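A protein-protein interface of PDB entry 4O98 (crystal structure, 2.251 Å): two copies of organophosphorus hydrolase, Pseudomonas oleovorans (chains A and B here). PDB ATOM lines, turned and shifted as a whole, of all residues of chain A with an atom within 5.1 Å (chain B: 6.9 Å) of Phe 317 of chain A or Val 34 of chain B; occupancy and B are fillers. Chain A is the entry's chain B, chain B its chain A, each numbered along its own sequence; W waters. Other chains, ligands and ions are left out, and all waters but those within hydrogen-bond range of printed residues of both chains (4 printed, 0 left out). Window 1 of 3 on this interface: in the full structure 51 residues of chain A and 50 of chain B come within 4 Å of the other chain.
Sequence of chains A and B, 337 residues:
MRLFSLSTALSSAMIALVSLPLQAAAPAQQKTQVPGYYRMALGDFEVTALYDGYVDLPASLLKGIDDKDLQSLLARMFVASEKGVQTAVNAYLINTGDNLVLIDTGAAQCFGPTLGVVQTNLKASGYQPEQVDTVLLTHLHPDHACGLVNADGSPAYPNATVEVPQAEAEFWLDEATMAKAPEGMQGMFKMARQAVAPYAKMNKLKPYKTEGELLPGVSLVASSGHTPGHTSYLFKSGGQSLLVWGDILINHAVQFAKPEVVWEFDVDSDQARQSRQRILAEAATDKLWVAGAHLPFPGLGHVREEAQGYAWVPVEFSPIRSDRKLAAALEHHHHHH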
ATOM      1  N   VAL A  34      19.767  11.627 -20.380  1.00  0.00           N
ATOM      2  CA  VAL A  34      20.624  12.790 -20.573  1.00  0.00           C
ATOM      3  C   VAL A  34      21.997  12.494 -19.944  1.00  0.00           C
ATOM      4  O   VAL A  34      22.087  11.762 -18.947  1.00  0.00           O
ATOM      5  CB  VAL A  34      19.975  14.058 -19.938  1.00  0.00           C
ATOM      6  CG1 VAL A  34      19.850  13.908 -18.429  1.00  0.00           C
ATOM      7  CG2 VAL A  34      20.750  15.324 -20.282  1.00  0.00           C
ATOM      8  N   PRO A  35      23.073  13.014 -20.555  1.00  0.00           N
ATOM      9  CA  PRO A  35      24.407  12.803 -19.992  1.00  0.00           C
ATOM     10  C   PRO A  35      24.522  13.235 -18.536  1.00  0.00           C
ATOM     11  O   PRO A  35      23.935  14.251 -18.131  1.00  0.00           O
ATOM     12  CB  PRO A  35      25.280  13.686 -20.881  1.00  0.00           C
ATOM     13  CG  PRO A  35      24.621  13.534 -22.243  1.00  0.00           C
ATOM     14  CD  PRO A  35      23.143  13.542 -21.938  1.00  0.00           C
ATOM     15  N   TYR A  37      26.327  15.004 -16.543  1.00  0.00           N
ATOM     16  CA  TYR A  37      27.142  16.135 -16.093  1.00  0.00           C
ATOM     17  C   TYR A  37      26.234  17.319 -15.793  1.00  0.00           C
ATOM     18  O   TYR A  37      25.113  17.398 -16.305  1.00  0.00           O
ATOM     19  CB  TYR A  37      28.273  16.504 -17.071  1.00  0.00           C
ATOM     20  CG  TYR A  37      27.817  17.114 -18.389  1.00  0.00           C
ATOM     21  CD1 TYR A  37      27.519  16.308 -19.477  1.00  0.00           C
ATOM     22  CD2 TYR A  37      27.715  18.495 -18.551  1.00  0.00           C
ATOM     23  CE1 TYR A  37      27.115  16.848 -20.681  1.00  0.00           C
ATOM     24  CE2 TYR A  37      27.299  19.049 -19.761  1.00  0.00           C
ATOM     25  CZ  TYR A  37      27.007  18.215 -20.818  1.00  0.00           C
ATOM     26  OH  TYR A  37      26.587  18.731 -22.025  1.00  0.00           O
ATOM     27  N   TYR A  38      26.700  18.208 -14.922  1.00  0.00           N
ATOM     28  CA  TYR A  38      25.915  19.367 -14.510  1.00  0.00           C
ATOM     29  C   TYR A  38      26.859  20.463 -14.061  1.00  0.00           C
ATOM     30  O   TYR A  38      27.753  20.219 -13.243  1.00  0.00           O
ATOM     31  CB  TYR A  38      24.954  19.034 -13.360  1.00  0.00           C
ATOM     32  CG  TYR A  38      24.118  20.237 -12.970  1.00  0.00           C
ATOM     33  CD1 TYR A  38      22.994  20.594 -13.710  1.00  0.00           C
ATOM     34  CD2 TYR A  38      24.475  21.033 -11.888  1.00  0.00           C
ATOM     35  CE1 TYR A  38      22.234  21.702 -13.368  1.00  0.00           C
ATOM     36  CE2 TYR A  38      23.725  22.146 -11.532  1.00  0.00           C
ATOM     37  CZ  TYR A  38      22.607  22.477 -12.271  1.00  0.00           C
ATOM     38  OH  TYR A  38      21.860  23.583 -11.924  1.00  0.00           O
ATOM     39  N   VAL A 315      20.235  21.707  -5.282  1.00  0.00           N
ATOM     40  CA  VAL A 315      20.254  22.849  -6.194  1.00  0.00           C
ATOM     41  C   VAL A 315      19.124  22.732  -7.217  1.00  0.00           C
ATOM     42  O   VAL A 315      18.765  21.619  -7.624  1.00  0.00           O
ATOM     43  CB  VAL A 315      21.597  22.956  -6.953  1.00  0.00           C
ATOM     44  CG1 VAL A 315      21.748  21.814  -7.963  1.00  0.00           C
ATOM     45  CG2 VAL A 315      21.696  24.290  -7.680  1.00  0.00           C
ATOM     46  N   GLU A 316      18.551  23.870  -7.619  1.00  0.00           N
ATOM     47  CA  GLU A 316      17.574  23.886  -8.701  1.00  0.00           C
ATOM     48  C   GLU A 316      18.285  23.978 -10.048  1.00  0.00           C
ATOM     49  O   GLU A 316      19.213  24.774 -10.205  1.00  0.00           O
ATOM     50  CB  GLU A 316      16.609  25.069  -8.543  1.00  0.00           C
ATOM     51  CG  GLU A 316      15.881  25.058  -7.234  1.00  0.00           C
ATOM     52  CD  GLU A 316      14.835  26.149  -7.122  1.00  0.00           C
ATOM     53  OE1 GLU A 316      14.479  26.759  -8.150  1.00  0.00           O
ATOM     54  OE2 GLU A 316      14.363  26.390  -5.992  1.00  0.00           O
ATOM     55  N   PHE A 317      17.836  23.183 -11.017  1.00  0.00           N
ATOM     56  CA  PHE A 317      18.418  23.198 -12.353  1.00  0.00           C
ATOM     57  C   PHE A 317      18.401  24.605 -12.945  1.00  0.00           C
ATOM     58  O   PHE A 317      17.345  25.259 -12.996  1.00  0.00           O
ATOM     59  CB  PHE A 317      17.659  22.251 -13.274  1.00  0.00           C
ATOM     60  CG  PHE A 317      18.292  22.085 -14.632  1.00  0.00           C
ATOM     61  CD1 PHE A 317      17.942  22.923 -15.684  1.00  0.00           C
ATOM     62  CD2 PHE A 317      19.230  21.084 -14.858  1.00  0.00           C
ATOM     63  CE1 PHE A 317      18.525  22.776 -16.955  1.00  0.00           C
ATOM     64  CE2 PHE A 317      19.818  20.925 -16.120  1.00  0.00           C
ATOM     65  CZ  PHE A 317      19.466  21.768 -17.171  1.00  0.00           C
ATOM     66  N   SER A 318      19.574  25.057 -13.387  1.00  0.00           N
ATOM     67  CA  SER A 318      19.737  26.411 -13.918  1.00  0.00           C
ATOM     68  C   SER A 318      20.951  26.523 -14.813  1.00  0.00           C
ATOM     69  O   SER A 318      21.986  25.921 -14.549  1.00  0.00           O
ATOM     70  CB  SER A 318      19.915  27.427 -12.789  1.00  0.00           C
ATOM     71  OG  SER A 318      20.160  28.720 -13.339  1.00  0.00           O
ATOM     72  N   PRO A 319      20.830  27.312 -15.883  1.00  0.00           N
ATOM     73  CA  PRO A 319      22.051  27.735 -16.573  1.00  0.00           C
ATOM     74  C   PRO A 319      22.837  28.634 -15.614  1.00  0.00           C
ATOM     75  O   PRO A 319      22.282  29.149 -14.641  1.00  0.00           O
ATOM     76  CB  PRO A 319      21.527  28.570 -17.751  1.00  0.00           C
ATOM     77  CG  PRO A 319      20.047  28.192 -17.893  1.00  0.00           C
ATOM     78  CD  PRO A 319      19.598  27.841 -16.501  1.00  0.00           C
ATOM     79  N   LYS B  31      31.698  26.244 -19.380  1.00  0.00           N
ATOM     80  CA  LYS B  31      30.492  27.045 -19.128  1.00  0.00           C
ATOM     81  C   LYS B  31      29.127  26.390 -19.457  1.00  0.00           C
ATOM     82  O   LYS B  31      28.229  26.378 -18.611  1.00  0.00           O
ATOM     83  CB  LYS B  31      30.583  28.407 -19.831  1.00  0.00           C
ATOM     84  CG  LYS B  31      31.817  29.251 -19.483  1.00  0.00           C
ATOM     85  CD  LYS B  31      31.817  30.553 -20.320  1.00  0.00           C
ATOM     86  CE  LYS B  31      32.988  31.470 -19.953  1.00  0.00           C
ATOM     87  NZ  LYS B  31      34.114  31.408 -20.936  1.00  0.00           N
ATOM     88  N   THR B  32      28.961  25.888 -20.679  1.00  0.00           N
ATOM     89  CA  THR B  32      27.654  25.421 -21.147  1.00  0.00           C
ATOM     90  C   THR B  32      27.025  24.385 -20.213  1.00  0.00           C
ATOM     91  O   THR B  32      27.728  23.570 -19.602  1.00  0.00           O
ATOM     92  CB  THR B  32      27.739  24.834 -22.566  1.00  0.00           C
ATOM     93  OG1 THR B  32      28.664  23.741 -22.567  1.00  0.00           O
ATOM     94  CG2 THR B  32      28.235  25.881 -23.541  1.00  0.00           C
ATOM     95  N   GLN B  33      25.702  24.431 -20.101  1.00  0.00           N
ATOM     96  CA  GLN B  33      24.973  23.553 -19.202  1.00  0.00           C
ATOM     97  C   GLN B  33      24.563  22.298 -19.950  1.00  0.00           C
ATOM     98  O   GLN B  33      24.397  22.328 -21.167  1.00  0.00           O
ATOM     99  CB  GLN B  33      23.726  24.271 -18.684  1.00  0.00           C
ATOM    100  CG  GLN B  33      22.908  23.490 -17.637  1.00  0.00           C
ATOM    101  CD  GLN B  33      23.742  23.087 -16.441  1.00  0.00           C
ATOM    102  OE1 GLN B  33      24.487  22.102 -16.492  1.00  0.00           O
ATOM    103  NE2 GLN B  33      23.643  23.860 -15.359  1.00  0.00           N
ATOM    104  N   VAL B  34      24.379  21.198 -19.224  1.00  0.00           N
ATOM    105  CA  VAL B  34      23.852  19.976 -19.831  1.00  0.00           C
ATOM    106  C   VAL B  34      22.522  20.323 -20.520  1.00  0.00           C
ATOM    107  O   VAL B  34      21.854  21.268 -20.107  1.00  0.00           O
ATOM    108  CB  VAL B  34      23.667  18.873 -18.752  1.00  0.00           C
ATOM    109  CG1 VAL B  34      22.523  19.229 -17.800  1.00  0.00           C
ATOM    110  CG2 VAL B  34      23.435  17.500 -19.389  1.00  0.00           C
ATOM    111  N   PRO B  35      22.164  19.618 -21.609  1.00  0.00           N
ATOM    112  CA  PRO B  35      20.866  19.902 -22.233  1.00  0.00           C
ATOM    113  C   PRO B  35      19.689  19.745 -21.288  1.00  0.00           C
ATOM    114  O   PRO B  35      19.753  18.947 -20.347  1.00  0.00           O
ATOM    115  CB  PRO B  35      20.778  18.839 -23.334  1.00  0.00           C
ATOM    116  CG  PRO B  35      22.182  18.665 -23.767  1.00  0.00           C
ATOM    117  CD  PRO B  35      23.030  18.831 -22.509  1.00  0.00           C
ATOM    118  N   GLY B  36      18.613  20.478 -21.557  1.00  0.00           N
ATOM    119  CA  GLY B  36      17.449  20.455 -20.695  1.00  0.00           C
ATOM    120  C   GLY B  36      16.422  19.385 -21.043  1.00  0.00           C
ATOM    121  O   GLY B  36      15.249  19.704 -21.319  1.00  0.00           O
ATOM    122  N   TYR B  37      16.847  18.122 -21.043  1.00  0.00           N
ATOM    123  CA  TYR B  37      15.886  17.022 -21.123  1.00  0.00           C
ATOM    124  C   TYR B  37      16.216  15.993 -20.050  1.00  0.00           C
ATOM    125  O   TYR B  37      17.351  15.950 -19.557  1.00  0.00           O
ATOM    126  CB  TYR B  37      15.800  16.395 -22.531  1.00  0.00           C
ATOM    127  CG  TYR B  37      17.017  15.611 -22.972  1.00  0.00           C
ATOM    128  CD1 TYR B  37      17.124  14.246 -22.720  1.00  0.00           C
ATOM    129  CD2 TYR B  37      18.047  16.230 -23.661  1.00  0.00           C
ATOM    130  CE1 TYR B  37      18.242  13.523 -23.129  1.00  0.00           C
ATOM    131  CE2 TYR B  37      19.154  15.529 -24.065  1.00  0.00           C
ATOM    132  CZ  TYR B  37      19.249  14.178 -23.800  1.00  0.00           C
ATOM    133  OH  TYR B  37      20.372  13.497 -24.207  1.00  0.00           O
ATOM    134  N   TYR B  51      13.018  21.289 -20.718  1.00  0.00           N
ATOM    135  CA  TYR B  51      13.250  22.600 -20.112  1.00  0.00           C
ATOM    136  C   TYR B  51      13.039  23.719 -21.135  1.00  0.00           C
ATOM    137  O   TYR B  51      13.649  23.693 -22.216  1.00  0.00           O
ATOM    138  CB  TYR B  51      14.688  22.646 -19.607  1.00  0.00           C
ATOM    139  CG  TYR B  51      15.098  23.885 -18.830  1.00  0.00           C
ATOM    140  CD1 TYR B  51      14.447  24.245 -17.652  1.00  0.00           C
ATOM    141  CD2 TYR B  51      16.182  24.660 -19.243  1.00  0.00           C
ATOM    142  CE1 TYR B  51      14.838  25.369 -16.924  1.00  0.00           C
ATOM    143  CE2 TYR B  51      16.595  25.781 -18.515  1.00  0.00           C
ATOM    144  CZ  TYR B  51      15.916  26.133 -17.363  1.00  0.00           C
ATOM    145  OH  TYR B  51      16.312  27.237 -16.637  1.00  0.00           O
ATOM    146  N   TYR B  54      14.060  29.869 -18.139  1.00  0.00           N
ATOM    147  CA  TYR B  54      13.626  30.441 -16.870  1.00  0.00           C
ATOM    148  C   TYR B  54      13.050  31.833 -17.064  1.00  0.00           C
ATOM    149  O   TYR B  54      13.310  32.483 -18.084  1.00  0.00           O
ATOM    150  CB  TYR B  54      14.802  30.498 -15.889  1.00  0.00           C
ATOM    151  CG  TYR B  54      15.942  31.398 -16.347  1.00  0.00           C
ATOM    152  CD1 TYR B  54      15.923  32.762 -16.083  1.00  0.00           C
ATOM    153  CD2 TYR B  54      17.031  30.881 -17.045  1.00  0.00           C
ATOM    154  CE1 TYR B  54      16.949  33.594 -16.500  1.00  0.00           C
ATOM    155  CE2 TYR B  54      18.065  31.708 -17.464  1.00  0.00           C
ATOM    156  CZ  TYR B  54      18.017  33.065 -17.185  1.00  0.00           C
ATOM    157  OH  TYR B  54      19.046  33.898 -17.591  1.00  0.00           O
ATOM    158  N   GLN B  86      13.890  33.201  -9.710  1.00  0.00           N
ATOM    159  CA  GLN B  86      14.114  32.506 -10.976  1.00  0.00           C
ATOM    160  C   GLN B  86      13.238  31.263 -11.032  1.00  0.00           C
ATOM    161  O   GLN B  86      13.327  30.386 -10.167  1.00  0.00           O
ATOM    162  CB  GLN B  86      15.583  32.110 -11.152  1.00  0.00           C
ATOM    163  CG  GLN B  86      15.850  31.347 -12.446  1.00  0.00           C
ATOM    164  CD  GLN B  86      17.305  30.961 -12.611  1.00  0.00           C
ATOM    165  OE1 GLN B  86      18.198  31.646 -12.117  1.00  0.00           O
ATOM    166  NE2 GLN B  86      17.552  29.861 -13.316  1.00  0.00           N
ATOM    167  N   ALA B  88      11.435  28.064 -13.289  1.00  0.00           N
ATOM    168  CA  ALA B  88      11.522  27.200 -14.473  1.00  0.00           C
ATOM    169  C   ALA B  88      10.203  27.163 -15.243  1.00  0.00           C
ATOM    170  O   ALA B  88       9.131  27.369 -14.665  1.00  0.00           O
ATOM    171  CB  ALA B  88      11.953  25.775 -14.084  1.00  0.00           C
ATOM    172  N   ASN B 121      15.458  21.320 -26.896  1.00  0.00           N
ATOM    173  CA  ASN B 121      15.667  20.199 -25.989  1.00  0.00           C
ATOM    174  C   ASN B 121      14.942  18.939 -26.463  1.00  0.00           C
ATOM    175  O   ASN B 121      15.415  17.829 -26.230  1.00  0.00           O
ATOM    176  CB  ASN B 121      15.288  20.578 -24.555  1.00  0.00           C
ATOM    177  CG  ASN B 121      16.370  21.391 -23.877  1.00  0.00           C
ATOM    178  OD1 ASN B 121      17.544  21.041 -23.960  1.00  0.00           O
ATOM    179  ND2 ASN B 121      15.988  22.493 -23.218  1.00  0.00           N
ATOM    180  N   PRO B 296      11.024  23.041 -10.137  1.00  0.00           N
ATOM    181  CA  PRO B 296      12.409  23.030 -10.618  1.00  0.00           C
ATOM    182  C   PRO B 296      12.601  21.863 -11.585  1.00  0.00           C
ATOM    183  O   PRO B 296      12.169  20.754 -11.259  1.00  0.00           O
ATOM    184  CB  PRO B 296      13.217  22.785  -9.340  1.00  0.00           C
ATOM    185  CG  PRO B 296      12.356  23.373  -8.244  1.00  0.00           C
ATOM    186  CD  PRO B 296      10.939  23.094  -8.665  1.00  0.00           C
ATOM    187  N   PHE B 297      13.230  22.115 -12.737  1.00  0.00           N
ATOM    188  CA  PHE B 297      13.408  21.108 -13.774  1.00  0.00           C
ATOM    189  C   PHE B 297      14.176  19.917 -13.211  1.00  0.00           C
ATOM    190  O   PHE B 297      15.181  20.111 -12.513  1.00  0.00           O
ATOM    191  CB  PHE B 297      14.150  21.704 -14.984  1.00  0.00           C
ATOM    192  CG  PHE B 297      14.342  20.717 -16.100  1.00  0.00           C
ATOM    193  CD1 PHE B 297      13.339  20.517 -17.038  1.00  0.00           C
ATOM    194  CD2 PHE B 297      15.503  19.942 -16.178  1.00  0.00           C
ATOM    195  CE1 PHE B 297      13.489  19.575 -18.043  1.00  0.00           C
ATOM    196  CE2 PHE B 297      15.659  18.996 -17.190  1.00  0.00           C
ATOM    197  CZ  PHE B 297      14.652  18.820 -18.124  1.00  0.00           C
ATOM    198  N   PRO B 298      13.753  18.679 -13.537  1.00  0.00           N
ATOM    199  CA  PRO B 298      12.736  18.259 -14.518  1.00  0.00           C
ATOM    200  C   PRO B 298      11.278  18.411 -14.085  1.00  0.00           C
ATOM    201  O   PRO B 298      10.377  18.119 -14.883  1.00  0.00           O
ATOM    202  CB  PRO B 298      13.053  16.773 -14.745  1.00  0.00           C
ATOM    203  CG  PRO B 298      13.686  16.314 -13.417  1.00  0.00           C
ATOM    204  CD  PRO B 298      14.437  17.531 -12.897  1.00  0.00           C
HETATM  205  O   HOH W   1      16.014  27.359 -14.052  1.00  0.00           O
HETATM  206  O   HOH W   2      14.829  30.142  -8.058  1.00  0.00           O
HETATM  207  O   HOH W   3      14.889  24.679 -12.428  1.00  0.00           O
HETATM  208  O   HOH W   4      16.124  21.110 -10.369  1.00  0.00           O
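The side-chain amide nitrogen (NE2) of Gln 33 of chain B sits at hydrogen-bond distance from the backbone carbonyl oxygen (O) of Ser 318 of chain A, 2.8 Å away.
The side-chain hydroxyl of Ser 318 of chain A lies within hydrogen-bond range of the side-chain amide nitrogen of Gln 86 of chain B, 2.8 Å away.
The backbone NH of Tyr 51 of chain B lies within hydrogen-bond range of the backbone carbonyl oxygen of Gly 36 of chain B, 2.8 Å away.
The backbone carbonyl oxygen (O) of Tyr 51 of chain B is in hydrogen-bond range of the side-chain amide nitrogen (ND2) of Asn 121 of chain B (2.8 Å).
OH of Tyr 38 of chain A lies within hydrogen-bond range of O of Glu 316 of chain A (3.4 Å).
OH of Tyr 38 of chain A sits at hydrogen-bond distance from N of Ser 318 of chain A, at 3.1 Å.
Among the printed residues, pairs that only touch across the chains: Tyr 37 of chain A with Val 34 of chain B (3.2 Å), Tyr 38 of chain A with Gln 33 of chain B (3.3 Å), Val 34 of chain A with Tyr 37 of chain B (3.3 Å), Pro 319 of chain A with Tyr 51 of chain B (3.3 Å), Phe 317 of chain A with Phe 297 of chain B (3.4 Å), Pro 35 of chain A with Val 34 of chain B (3.5 Å), Val 34 of chain A with Val 34 of chain B (3.6 Å), Pro 35 of chain A with Tyr 37 of chain B (3.6 Å), Tyr 37 of chain A with Pro 35 of chain B (3.6 Å), Phe 317 of chain A with Val 34 of chain B (3.6 Å), Val 34 of chain A with Pro 35 of chain B (3.8 Å), Phe 317 of chain A with Tyr 51 of chain B (3.8 Å), Phe 317 of chain A with Gln 33 of chain B (3.9 Å) and Glu 316 of chain A with Pro 296 of chain B (3.9 Å).
Printed residues of chain B within 4 Å of Tyr 38 of chain A: Gln 33 (3.3 Å).
Of chain B, only Gln 33 (3.9 Å), Val 34 (3.6 Å), Tyr 51 (3.8 Å) and Phe 297 (3.4 Å) come within 4 Å of Phe 317 of chain A.
Of the printed residues of chain B, Ser 318 of chain A touches Gln 33 and Gln 86.
Lys 31 of chain B touches none of the printed residues of chain A.
Of the printed residues of chain A, Gln 33 of chain B touches Tyr 38, Phe 317 and Ser 318.
Val 34 of chain B touches just these residues of chain A: Val 34 (3.6 Å), Pro 35 (3.5 Å), Tyr 37 (3.2 Å) and Phe 317 (3.6 Å).
Of the printed residues of chain A, Pro 296 of chain B touches Glu 316.
Pro 298 of chain B touches none of the printed residues of chain A.
Printed residues of chain B that touch a printed residue of chain A: Gln 33, Val 34, Pro 35, Tyr 37, Tyr 51, Gln 86, Pro 296 and Phe 297.
Hydrophobic or aromatic side chains of chain B within 4 Å of the printed part of chain A: Val 34, Pro 35, Tyr 37, Tyr 51, Pro 296 and Phe 297.
Among the printed residues, no Asp or Glu carboxylate lies within 4 Å of a Lys or Arg side-chain nitrogen of the other chain.
Val 34 of chain A touches its own counterpart, Val 34 of chain B.
Val 34 of chain A touches Pro 35 of chain B, and with the chains exchanged Pro 35 of chain A touches Val 34 of chain B.
Val 34 of chain A touches Tyr 37 of chain B, and with the chains exchanged Tyr 37 of chain A touches Val 34 of chain B.
Pro 35 of chain A touches Tyr 37 of chain B, and with the chains exchanged Tyr 37 of chain A touches Pro 35 of chain B.
Positions printed for both chains: 34, 35 and 37.
Water W4 lies within hydrogen-bond range of the backbone carbonyl oxygen (O) of Phe 297 of chain B (2.5 Å) and the backbone NH (N) of Phe 317 of chain A (2.8 Å).
Water W3 lies within hydrogen-bond range of the backbone carbonyl oxygen of Phe 317 of chain A (2.6 Å) and the backbone NH of Phe 297 of chain B (3.1 Å).
Water W2 lies within hydrogen-bond range of the backbone carbonyl oxygen of Gln 86 of chain B (2.6 Å) and the side-chain carboxylate of Glu 316 of chain A (3.4 Å).
Water W1 lies within hydrogen-bond range of OH of Tyr 51 of chain B (2.6 Å), O of Phe 317 of chain A (2.7 Å) and NE2 of Gln 86 of chain B (3.0 Å).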
